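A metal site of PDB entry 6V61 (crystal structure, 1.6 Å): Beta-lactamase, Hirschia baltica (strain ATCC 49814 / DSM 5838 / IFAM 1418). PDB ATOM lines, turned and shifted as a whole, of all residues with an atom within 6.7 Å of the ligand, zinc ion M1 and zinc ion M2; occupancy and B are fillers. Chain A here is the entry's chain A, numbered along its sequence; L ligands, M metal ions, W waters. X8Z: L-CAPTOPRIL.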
ATOM      1  N   LYS A  35     -27.303 -13.505 -18.676  1.00  0.00           N
ATOM      2  CA  LYS A  35     -27.017 -13.809 -17.284  1.00  0.00           C
ATOM      3  C   LYS A  35     -25.538 -13.620 -17.061  1.00  0.00           C
ATOM      4  O   LYS A  35     -24.735 -14.045 -17.904  1.00  0.00           O
ATOM      5  CB  LYS A  35     -27.406 -15.237 -16.904  1.00  0.00           C
ATOM      6  CG  LYS A  35     -27.172 -15.579 -15.436  1.00  0.00           C
ATOM      7  CD  LYS A  35     -27.552 -17.037 -15.160  1.00  0.00           C
ATOM      8  CE  LYS A  35     -27.415 -17.360 -13.678  1.00  0.00           C
ATOM      9  NZ  LYS A  35     -27.909 -18.739 -13.369  1.00  0.00           N
ATOM     10  N   VAL A  37     -22.397 -14.824 -15.469  1.00  0.00           N
ATOM     11  CA  VAL A  37     -21.880 -16.078 -14.922  1.00  0.00           C
ATOM     12  C   VAL A  37     -20.383 -15.921 -14.709  1.00  0.00           C
ATOM     13  O   VAL A  37     -19.606 -15.976 -15.662  1.00  0.00           O
ATOM     14  CB  VAL A  37     -22.187 -17.248 -15.868  1.00  0.00           C
ATOM     15  CG1 VAL A  37     -21.653 -18.553 -15.267  1.00  0.00           C
ATOM     16  CG2 VAL A  37     -23.691 -17.334 -16.129  1.00  0.00           C
ATOM     17  N   ILE A  43     -23.619 -13.950 -20.495  1.00  0.00           N
ATOM     18  CA  ILE A  43     -23.765 -14.981 -21.518  1.00  0.00           C
ATOM     19  C   ILE A  43     -25.213 -14.997 -21.981  1.00  0.00           C
ATOM     20  O   ILE A  43     -26.137 -14.987 -21.161  1.00  0.00           O
ATOM     21  CB  ILE A  43     -23.328 -16.368 -20.997  1.00  0.00           C
ATOM     22  CG1 ILE A  43     -23.638 -17.450 -22.039  1.00  0.00           C
ATOM     23  CG2 ILE A  43     -23.976 -16.682 -19.668  1.00  0.00           C
ATOM     24  CD1 ILE A  43     -22.958 -17.207 -23.377  1.00  0.00           C
ATOM     25  N   ARG A  44     -25.397 -15.018 -23.298  1.00  0.00           N
ATOM     26  CA  ARG A  44     -26.723 -14.982 -23.911  1.00  0.00           C
ATOM     27  C   ARG A  44     -27.334 -16.374 -23.940  1.00  0.00           C
ATOM     28  O   ARG A  44     -26.632 -17.387 -23.974  1.00  0.00           O
ATOM     29  CB  ARG A  44     -26.661 -14.464 -25.358  1.00  0.00           C
ATOM     30  CG  ARG A  44     -26.083 -15.503 -26.350  1.00  0.00           C
ATOM     31  CD  ARG A  44     -25.849 -14.918 -27.723  1.00  0.00           C
ATOM     32  NE  ARG A  44     -27.099 -14.554 -28.379  1.00  0.00           N
ATOM     33  CZ  ARG A  44     -27.154 -13.754 -29.434  1.00  0.00           C
ATOM     34  NH1 ARG A  44     -26.033 -13.207 -29.935  1.00  0.00           N
ATOM     35  NH2 ARG A  44     -28.324 -13.444 -29.975  1.00  0.00           N
ATOM     36  N   THR A  45     -28.656 -16.403 -23.944  1.00  0.00           N
ATOM     37  CA  THR A  45     -29.391 -17.593 -24.357  1.00  0.00           C
ATOM     38  C   THR A  45     -30.492 -17.149 -25.296  1.00  0.00           C
ATOM     39  O   THR A  45     -31.125 -16.116 -25.073  1.00  0.00           O
ATOM     40  CB  THR A  45     -29.954 -18.391 -23.166  1.00  0.00           C
ATOM     41  OG1 THR A  45     -30.531 -19.630 -23.645  1.00  0.00           O
ATOM     42  CG2 THR A  45     -31.060 -17.624 -22.377  1.00  0.00           C
ATOM     43  N   TRP A  63     -33.605 -16.864 -19.071  1.00  0.00           N
ATOM     44  CA  TRP A  63     -32.903 -17.345 -17.890  1.00  0.00           C
ATOM     45  C   TRP A  63     -33.784 -17.407 -16.656  1.00  0.00           C
ATOM     46  O   TRP A  63     -33.481 -18.163 -15.717  1.00  0.00           O
ATOM     47  CB  TRP A  63     -31.699 -16.462 -17.576  1.00  0.00           C
ATOM     48  CG  TRP A  63     -30.560 -16.517 -18.571  1.00  0.00           C
ATOM     49  CD1 TRP A  63     -30.270 -15.579 -19.527  1.00  0.00           C
ATOM     50  CD2 TRP A  63     -29.542 -17.525 -18.668  1.00  0.00           C
ATOM     51  NE1 TRP A  63     -29.138 -15.961 -20.225  1.00  0.00           N
ATOM     52  CE2 TRP A  63     -28.681 -17.140 -19.717  1.00  0.00           C
ATOM     53  CE3 TRP A  63     -29.293 -18.713 -17.977  1.00  0.00           C
ATOM     54  CZ2 TRP A  63     -27.563 -17.908 -20.083  1.00  0.00           C
ATOM     55  CZ3 TRP A  63     -28.178 -19.466 -18.334  1.00  0.00           C
ATOM     56  CH2 TRP A  63     -27.331 -19.065 -19.382  1.00  0.00           C
ATOM     57  N   HIS A  90     -34.472 -28.622 -23.454  1.00  0.00           N
ATOM     58  CA  HIS A  90     -33.889 -29.562 -22.480  1.00  0.00           C
ATOM     59  C   HIS A  90     -33.981 -28.938 -21.091  1.00  0.00           C
ATOM     60  O   HIS A  90     -34.326 -27.755 -20.951  1.00  0.00           O
ATOM     61  CB  HIS A  90     -32.432 -29.999 -22.791  1.00  0.00           C
ATOM     62  CG  HIS A  90     -31.408 -28.908 -22.704  1.00  0.00           C
ATOM     63  ND1 HIS A  90     -31.254 -27.948 -23.676  1.00  0.00           N
ATOM     64  CD2 HIS A  90     -30.473 -28.629 -21.757  1.00  0.00           C
ATOM     65  CE1 HIS A  90     -30.277 -27.128 -23.340  1.00  0.00           C
ATOM     66  NE2 HIS A  90     -29.790 -27.513 -22.167  1.00  0.00           N
ATOM     67  N   ALA A  91     -33.642 -29.737 -20.072  1.00  0.00           N
ATOM     68  CA  ALA A  91     -33.892 -29.386 -18.669  1.00  0.00           C
ATOM     69  C   ALA A  91     -32.722 -28.616 -18.033  1.00  0.00           C
ATOM     70  O   ALA A  91     -32.153 -29.028 -17.009  1.00  0.00           O
ATOM     71  CB  ALA A  91     -34.203 -30.640 -17.868  1.00  0.00           C
ATOM     72  N   HIS A  92     -32.354 -27.485 -18.632  1.00  0.00           N
ATOM     73  CA  HIS A  92     -31.417 -26.565 -17.995  1.00  0.00           C
ATOM     74  C   HIS A  92     -32.074 -25.204 -17.815  1.00  0.00           C
ATOM     75  O   HIS A  92     -33.099 -24.888 -18.448  1.00  0.00           O
ATOM     76  CB  HIS A  92     -30.103 -26.428 -18.771  1.00  0.00           C
ATOM     77  CG  HIS A  92     -29.156 -27.568 -18.574  1.00  0.00           C
ATOM     78  ND1 HIS A  92     -28.230 -27.928 -19.542  1.00  0.00           N
ATOM     79  CD2 HIS A  92     -28.978 -28.428 -17.546  1.00  0.00           C
ATOM     80  CE1 HIS A  92     -27.518 -28.946 -19.105  1.00  0.00           C
ATOM     81  NE2 HIS A  92     -27.961 -29.285 -17.895  1.00  0.00           N
ATOM     82  N   SER A  93     -31.460 -24.380 -16.962  1.00  0.00           N
ATOM     83  CA  SER A  93     -32.131 -23.161 -16.519  1.00  0.00           C
ATOM     84  C   SER A  93     -32.166 -22.073 -17.593  1.00  0.00           C
ATOM     85  O   SER A  93     -32.968 -21.133 -17.479  1.00  0.00           O
ATOM     86  CB  SER A  93     -31.477 -22.627 -15.226  1.00  0.00           C
ATOM     87  OG  SER A  93     -30.199 -22.055 -15.460  1.00  0.00           O
ATOM     88  N   ASP A  94     -31.358 -22.170 -18.646  1.00  0.00           N
ATOM     89  CA  ASP A  94     -31.527 -21.213 -19.735  1.00  0.00           C
ATOM     90  C   ASP A  94     -32.752 -21.517 -20.611  1.00  0.00           C
ATOM     91  O   ASP A  94     -33.200 -20.638 -21.354  1.00  0.00           O
ATOM     92  CB  ASP A  94     -30.256 -21.130 -20.616  1.00  0.00           C
ATOM     93  CG  ASP A  94     -29.739 -22.468 -21.079  1.00  0.00           C
ATOM     94  OD1 ASP A  94     -30.117 -23.547 -20.567  1.00  0.00           O
ATOM     95  OD2 ASP A  94     -28.924 -22.396 -22.000  1.00  0.00           O
ATOM     96  N   LYS A  95     -33.278 -22.745 -20.551  1.00  0.00           N
ATOM     97  CA  LYS A  95     -34.427 -23.158 -21.348  1.00  0.00           C
ATOM     98  C   LYS A  95     -35.695 -23.294 -20.538  1.00  0.00           C
ATOM     99  O   LYS A  95     -36.788 -23.237 -21.114  1.00  0.00           O
ATOM    100  CB  LYS A  95     -34.148 -24.532 -22.013  1.00  0.00           C
ATOM    101  CG  LYS A  95     -32.720 -24.715 -22.528  1.00  0.00           C
ATOM    102  CD  LYS A  95     -32.517 -24.171 -23.935  1.00  0.00           C
ATOM    103  CE  LYS A  95     -32.319 -22.649 -24.000  1.00  0.00           C
ATOM    104  NZ  LYS A  95     -32.447 -22.132 -25.402  1.00  0.00           N
ATOM    105  N   HIS A 154     -25.583 -32.527 -26.333  1.00  0.00           N
ATOM    106  CA  HIS A 154     -25.328 -31.612 -25.231  1.00  0.00           C
ATOM    107  C   HIS A 154     -25.916 -32.153 -23.940  1.00  0.00           C
ATOM    108  O   HIS A 154     -25.310 -32.041 -22.853  1.00  0.00           O
ATOM    109  CB  HIS A 154     -25.929 -30.251 -25.549  1.00  0.00           C
ATOM    110  CG  HIS A 154     -26.098 -29.372 -24.338  1.00  0.00           C
ATOM    111  ND1 HIS A 154     -25.042 -28.705 -23.755  1.00  0.00           N
ATOM    112  CD2 HIS A 154     -27.186 -29.083 -23.599  1.00  0.00           C
ATOM    113  CE1 HIS A 154     -25.486 -28.031 -22.710  1.00  0.00           C
ATOM    114  NE2 HIS A 154     -26.783 -28.235 -22.594  1.00  0.00           N
ATOM    115  N   SER A 155     -27.099 -32.739 -24.035  1.00  0.00           N
ATOM    116  CA  SER A 155     -27.761 -33.403 -22.916  1.00  0.00           C
ATOM    117  C   SER A 155     -28.480 -34.645 -23.439  1.00  0.00           C
ATOM    118  O   SER A 155     -28.747 -34.760 -24.635  1.00  0.00           O
ATOM    119  CB  SER A 155     -28.755 -32.476 -22.242  1.00  0.00           C
ATOM    120  OG  SER A 155     -29.784 -32.165 -23.154  1.00  0.00           O
ATOM    121  N   GLY A 172     -30.776 -25.132 -30.466  1.00  0.00           N
ATOM    122  CA  GLY A 172     -30.613 -24.971 -29.025  1.00  0.00           C
ATOM    123  C   GLY A 172     -29.167 -25.197 -28.621  1.00  0.00           C
ATOM    124  O   GLY A 172     -28.226 -24.834 -29.344  1.00  0.00           O
ATOM    125  N   CYS A 173     -28.977 -25.782 -27.442  1.00  0.00           N
ATOM    126  CA  CYS A 173     -27.625 -25.875 -26.906  1.00  0.00           C
ATOM    127  C   CYS A 173     -26.869 -27.049 -27.502  1.00  0.00           C
ATOM    128  O   CYS A 173     -25.659 -27.159 -27.284  1.00  0.00           O
ATOM    129  CB  CYS A 173     -27.657 -25.985 -25.379  1.00  0.00           C
ATOM    130  SG  CYS A 173     -28.614 -24.623 -24.622  1.00  0.00           S
ATOM    131  N   ARG A 176     -23.185 -25.642 -31.142  1.00  0.00           N
ATOM    132  CA  ARG A 176     -22.265 -24.669 -30.584  1.00  0.00           C
ATOM    133  C   ARG A 176     -22.154 -23.458 -31.508  1.00  0.00           C
ATOM    134  O   ARG A 176     -22.359 -23.562 -32.721  1.00  0.00           O
ATOM    135  CB  ARG A 176     -20.893 -25.304 -30.381  1.00  0.00           C
ATOM    136  CG  ARG A 176     -20.928 -26.452 -29.367  1.00  0.00           C
ATOM    137  CD  ARG A 176     -21.211 -25.968 -27.923  1.00  0.00           C
ATOM    138  NE  ARG A 176     -20.159 -25.058 -27.462  1.00  0.00           N
ATOM    139  CZ  ARG A 176     -20.360 -24.000 -26.678  1.00  0.00           C
ATOM    140  NH1 ARG A 176     -21.589 -23.691 -26.259  1.00  0.00           N
ATOM    141  NH2 ARG A 176     -19.330 -23.235 -26.335  1.00  0.00           N
ATOM    142  N   LEU A 183     -16.826 -26.671 -25.870  1.00  0.00           N
ATOM    143  CA  LEU A 183     -18.035 -27.477 -25.867  1.00  0.00           C
ATOM    144  C   LEU A 183     -19.075 -26.980 -24.870  1.00  0.00           C
ATOM    145  O   LEU A 183     -20.164 -27.548 -24.807  1.00  0.00           O
ATOM    146  CB  LEU A 183     -17.701 -28.934 -25.556  1.00  0.00           C
ATOM    147  CG  LEU A 183     -16.673 -29.665 -26.420  1.00  0.00           C
ATOM    148  CD1 LEU A 183     -16.851 -31.162 -26.266  1.00  0.00           C
ATOM    149  CD2 LEU A 183     -16.808 -29.271 -27.881  1.00  0.00           C
ATOM    150  N   GLY A 184     -18.763 -25.926 -24.112  1.00  0.00           N
ATOM    151  CA  GLY A 184     -19.689 -25.499 -23.073  1.00  0.00           C
ATOM    152  C   GLY A 184     -19.587 -26.449 -21.896  1.00  0.00           C
ATOM    153  O   GLY A 184     -18.665 -27.238 -21.769  1.00  0.00           O
ATOM    154  N   ASN A 185     -20.624 -26.411 -21.050  1.00  0.00           N
ATOM    155  CA  ASN A 185     -20.658 -27.309 -19.904  1.00  0.00           C
ATOM    156  C   ASN A 185     -21.057 -28.709 -20.375  1.00  0.00           C
ATOM    157  O   ASN A 185     -22.138 -28.878 -20.963  1.00  0.00           O
ATOM    158  CB  ASN A 185     -21.615 -26.798 -18.831  1.00  0.00           C
ATOM    159  CG  ASN A 185     -21.543 -27.599 -17.551  1.00  0.00           C
ATOM    160  OD1 ASN A 185     -21.671 -28.824 -17.567  1.00  0.00           O
ATOM    161  ND2 ASN A 185     -21.320 -26.918 -16.430  1.00  0.00           N
ATOM    162  N   ILE A 186     -20.187 -29.675 -20.160  1.00  0.00           N
ATOM    163  CA  ILE A 186     -20.397 -31.025 -20.669  1.00  0.00           C
ATOM    164  C   ILE A 186     -20.639 -32.022 -19.547  1.00  0.00           C
ATOM    165  O   ILE A 186     -20.514 -33.220 -19.751  1.00  0.00           O
ATOM    166  CB  ILE A 186     -19.230 -31.469 -21.575  1.00  0.00           C
ATOM    167  CG1 ILE A 186     -17.893 -31.351 -20.839  1.00  0.00           C
ATOM    168  CG2 ILE A 186     -19.215 -30.645 -22.842  1.00  0.00           C
ATOM    169  CD1 ILE A 186     -16.786 -32.158 -21.500  1.00  0.00           C
ATOM    170  N   SER A 214     -28.248 -21.811 -29.036  1.00  0.00           N
ATOM    171  CA  SER A 214     -28.664 -21.045 -27.864  1.00  0.00           C
ATOM    172  C   SER A 214     -27.661 -19.958 -27.492  1.00  0.00           C
ATOM    173  O   SER A 214     -28.060 -18.900 -27.007  1.00  0.00           O
ATOM    174  CB  SER A 214     -28.882 -21.939 -26.644  1.00  0.00           C
ATOM    175  OG  SER A 214     -29.977 -22.791 -26.816  1.00  0.00           O
ATOM    176  N   HIS A 215     -26.365 -20.215 -27.649  1.00  0.00           N
ATOM    177  CA  HIS A 215     -25.369 -19.375 -26.987  1.00  0.00           C
ATOM    178  C   HIS A 215     -24.476 -18.605 -27.953  1.00  0.00           C
ATOM    179  O   HIS A 215     -23.346 -18.265 -27.629  1.00  0.00           O
ATOM    180  CB  HIS A 215     -24.526 -20.202 -26.014  1.00  0.00           C
ATOM    181  CG  HIS A 215     -25.337 -20.818 -24.923  1.00  0.00           C
ATOM    182  ND1 HIS A 215     -26.112 -20.060 -24.058  1.00  0.00           N
ATOM    183  CD2 HIS A 215     -25.560 -22.111 -24.580  1.00  0.00           C
ATOM    184  CE1 HIS A 215     -26.751 -20.850 -23.226  1.00  0.00           C
ATOM    185  NE2 HIS A 215     -26.422 -22.105 -23.511  1.00  0.00           N
HETATM  186  O1  X8Z L   1     -24.417 -24.950 -18.888  1.00  0.00           O
HETATM  187  C4  X8Z L   1     -24.793 -23.847 -19.279  1.00  0.00           C
HETATM  188  C2  X8Z L   1     -26.237 -23.484 -19.153  1.00  0.00           C
HETATM  189  C1  X8Z L   1     -27.086 -24.642 -19.668  1.00  0.00           C
HETATM  190  S   X8Z L   1     -26.690 -25.181 -21.361  1.00  0.00           S
HETATM  191  C3  X8Z L   1     -26.589 -23.160 -17.699  1.00  0.00           C
HETATM  192  N   X8Z L   1     -24.007 -22.908 -19.824  1.00  0.00           N
HETATM  193  C8  X8Z L   1     -23.022 -23.166 -20.868  1.00  0.00           C
HETATM  194  C9  X8Z L   1     -21.609 -23.145 -20.382  1.00  0.00           C
HETATM  195  O3  X8Z L   1     -21.364 -23.530 -19.215  1.00  0.00           O
HETATM  196  O2  X8Z L   1     -20.730 -22.726 -21.182  1.00  0.00           O
HETATM  197  C5  X8Z L   1     -24.057 -21.480 -19.530  1.00  0.00           C
HETATM  198  C6  X8Z L   1     -23.845 -20.889 -20.920  1.00  0.00           C
HETATM  199  C7  X8Z L   1     -23.160 -21.955 -21.766  1.00  0.00           C
HETATM  200 ZN    ZN M   1     -27.991 -27.108 -21.418  1.00  0.00          ZN
HETATM  201 ZN    ZN M   2     -27.654 -23.681 -22.815  1.00  0.00          ZN
HETATM  202  O   HOH W   1     -21.267 -21.346 -24.387  1.00  0.00           O
HETATM  203  O   HOH W   2     -24.299 -21.577 -15.590  1.00  0.00           O
HETATM  204  O   HOH W   3     -23.609 -25.122 -23.547  1.00  0.00           O
HETATM  205  O   HOH W   4     -22.669 -23.256 -17.020  1.00  0.00           O
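A ring nitrogen (NE2) of His 90 is bound to zinc ion M1, 2.0 Å away.
Zinc ion M1 is bound by NE2 of His 154, 2.0 Å away.
Zinc ion M1 is bound by a ring nitrogen (ND1) of His 92.
Zinc ion M1 is bound by a sulfur (S) of the ligand.
Zinc ion M1 has four donor atoms within binding distance.
Ile 43 touches the ligand.
Gly 184 touches the ligand (CA to O2, 3.5 Å).
Hydrophobic or aromatic side chains that line the ligand: Ile 43, His 92, His 154 and His 215.
The nearest printed residue that does not touch the ligand is Trp 63 (4.1 Å).
Within 4 Å of zinc ion M2: Asp 94, Cys 173 and His 215.
The nearest printed residue that does not touch zinc ion M2 is His 90 (4.4 Å).
The backbone NH of Asn 185 sits close to an oxygen (O3) of the ligand (3.5 Å).
A ring nitrogen (ND1) of His 215 is in hydrogen-bond range of the backbone carbonyl oxygen of Arg 44 (2.7 Å).
The backbone NH (N) of Cys 173 lies within hydrogen-bond range of the side-chain hydroxyl (OG) of Ser 214, 3.2 Å away.
O of Ile 43 lies within hydrogen-bond range of NE1 of Trp 63.
The backbone NH (N) of Ile 43 sits at hydrogen-bond distance from the backbone carbonyl oxygen (O) of Lys 35, 2.8 Å away.
Of the 23 residues printed, 3 come within 4 Å of zinc ion M1.
Along chain A the residues within 4 Å of zinc ion M1 span positions 90 to 154.
Zinc ion M2 is bound by OD2 of Asp 94, 2.0 Å away.
NE2 of His 215 is bound to zinc ion M2 (2.1 Å).
SG of Cys 173 binds zinc ion M2 (2.3 Å).
Zinc ion M2 is bound by a sulfur (S) of the ligand (2.3 Å).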
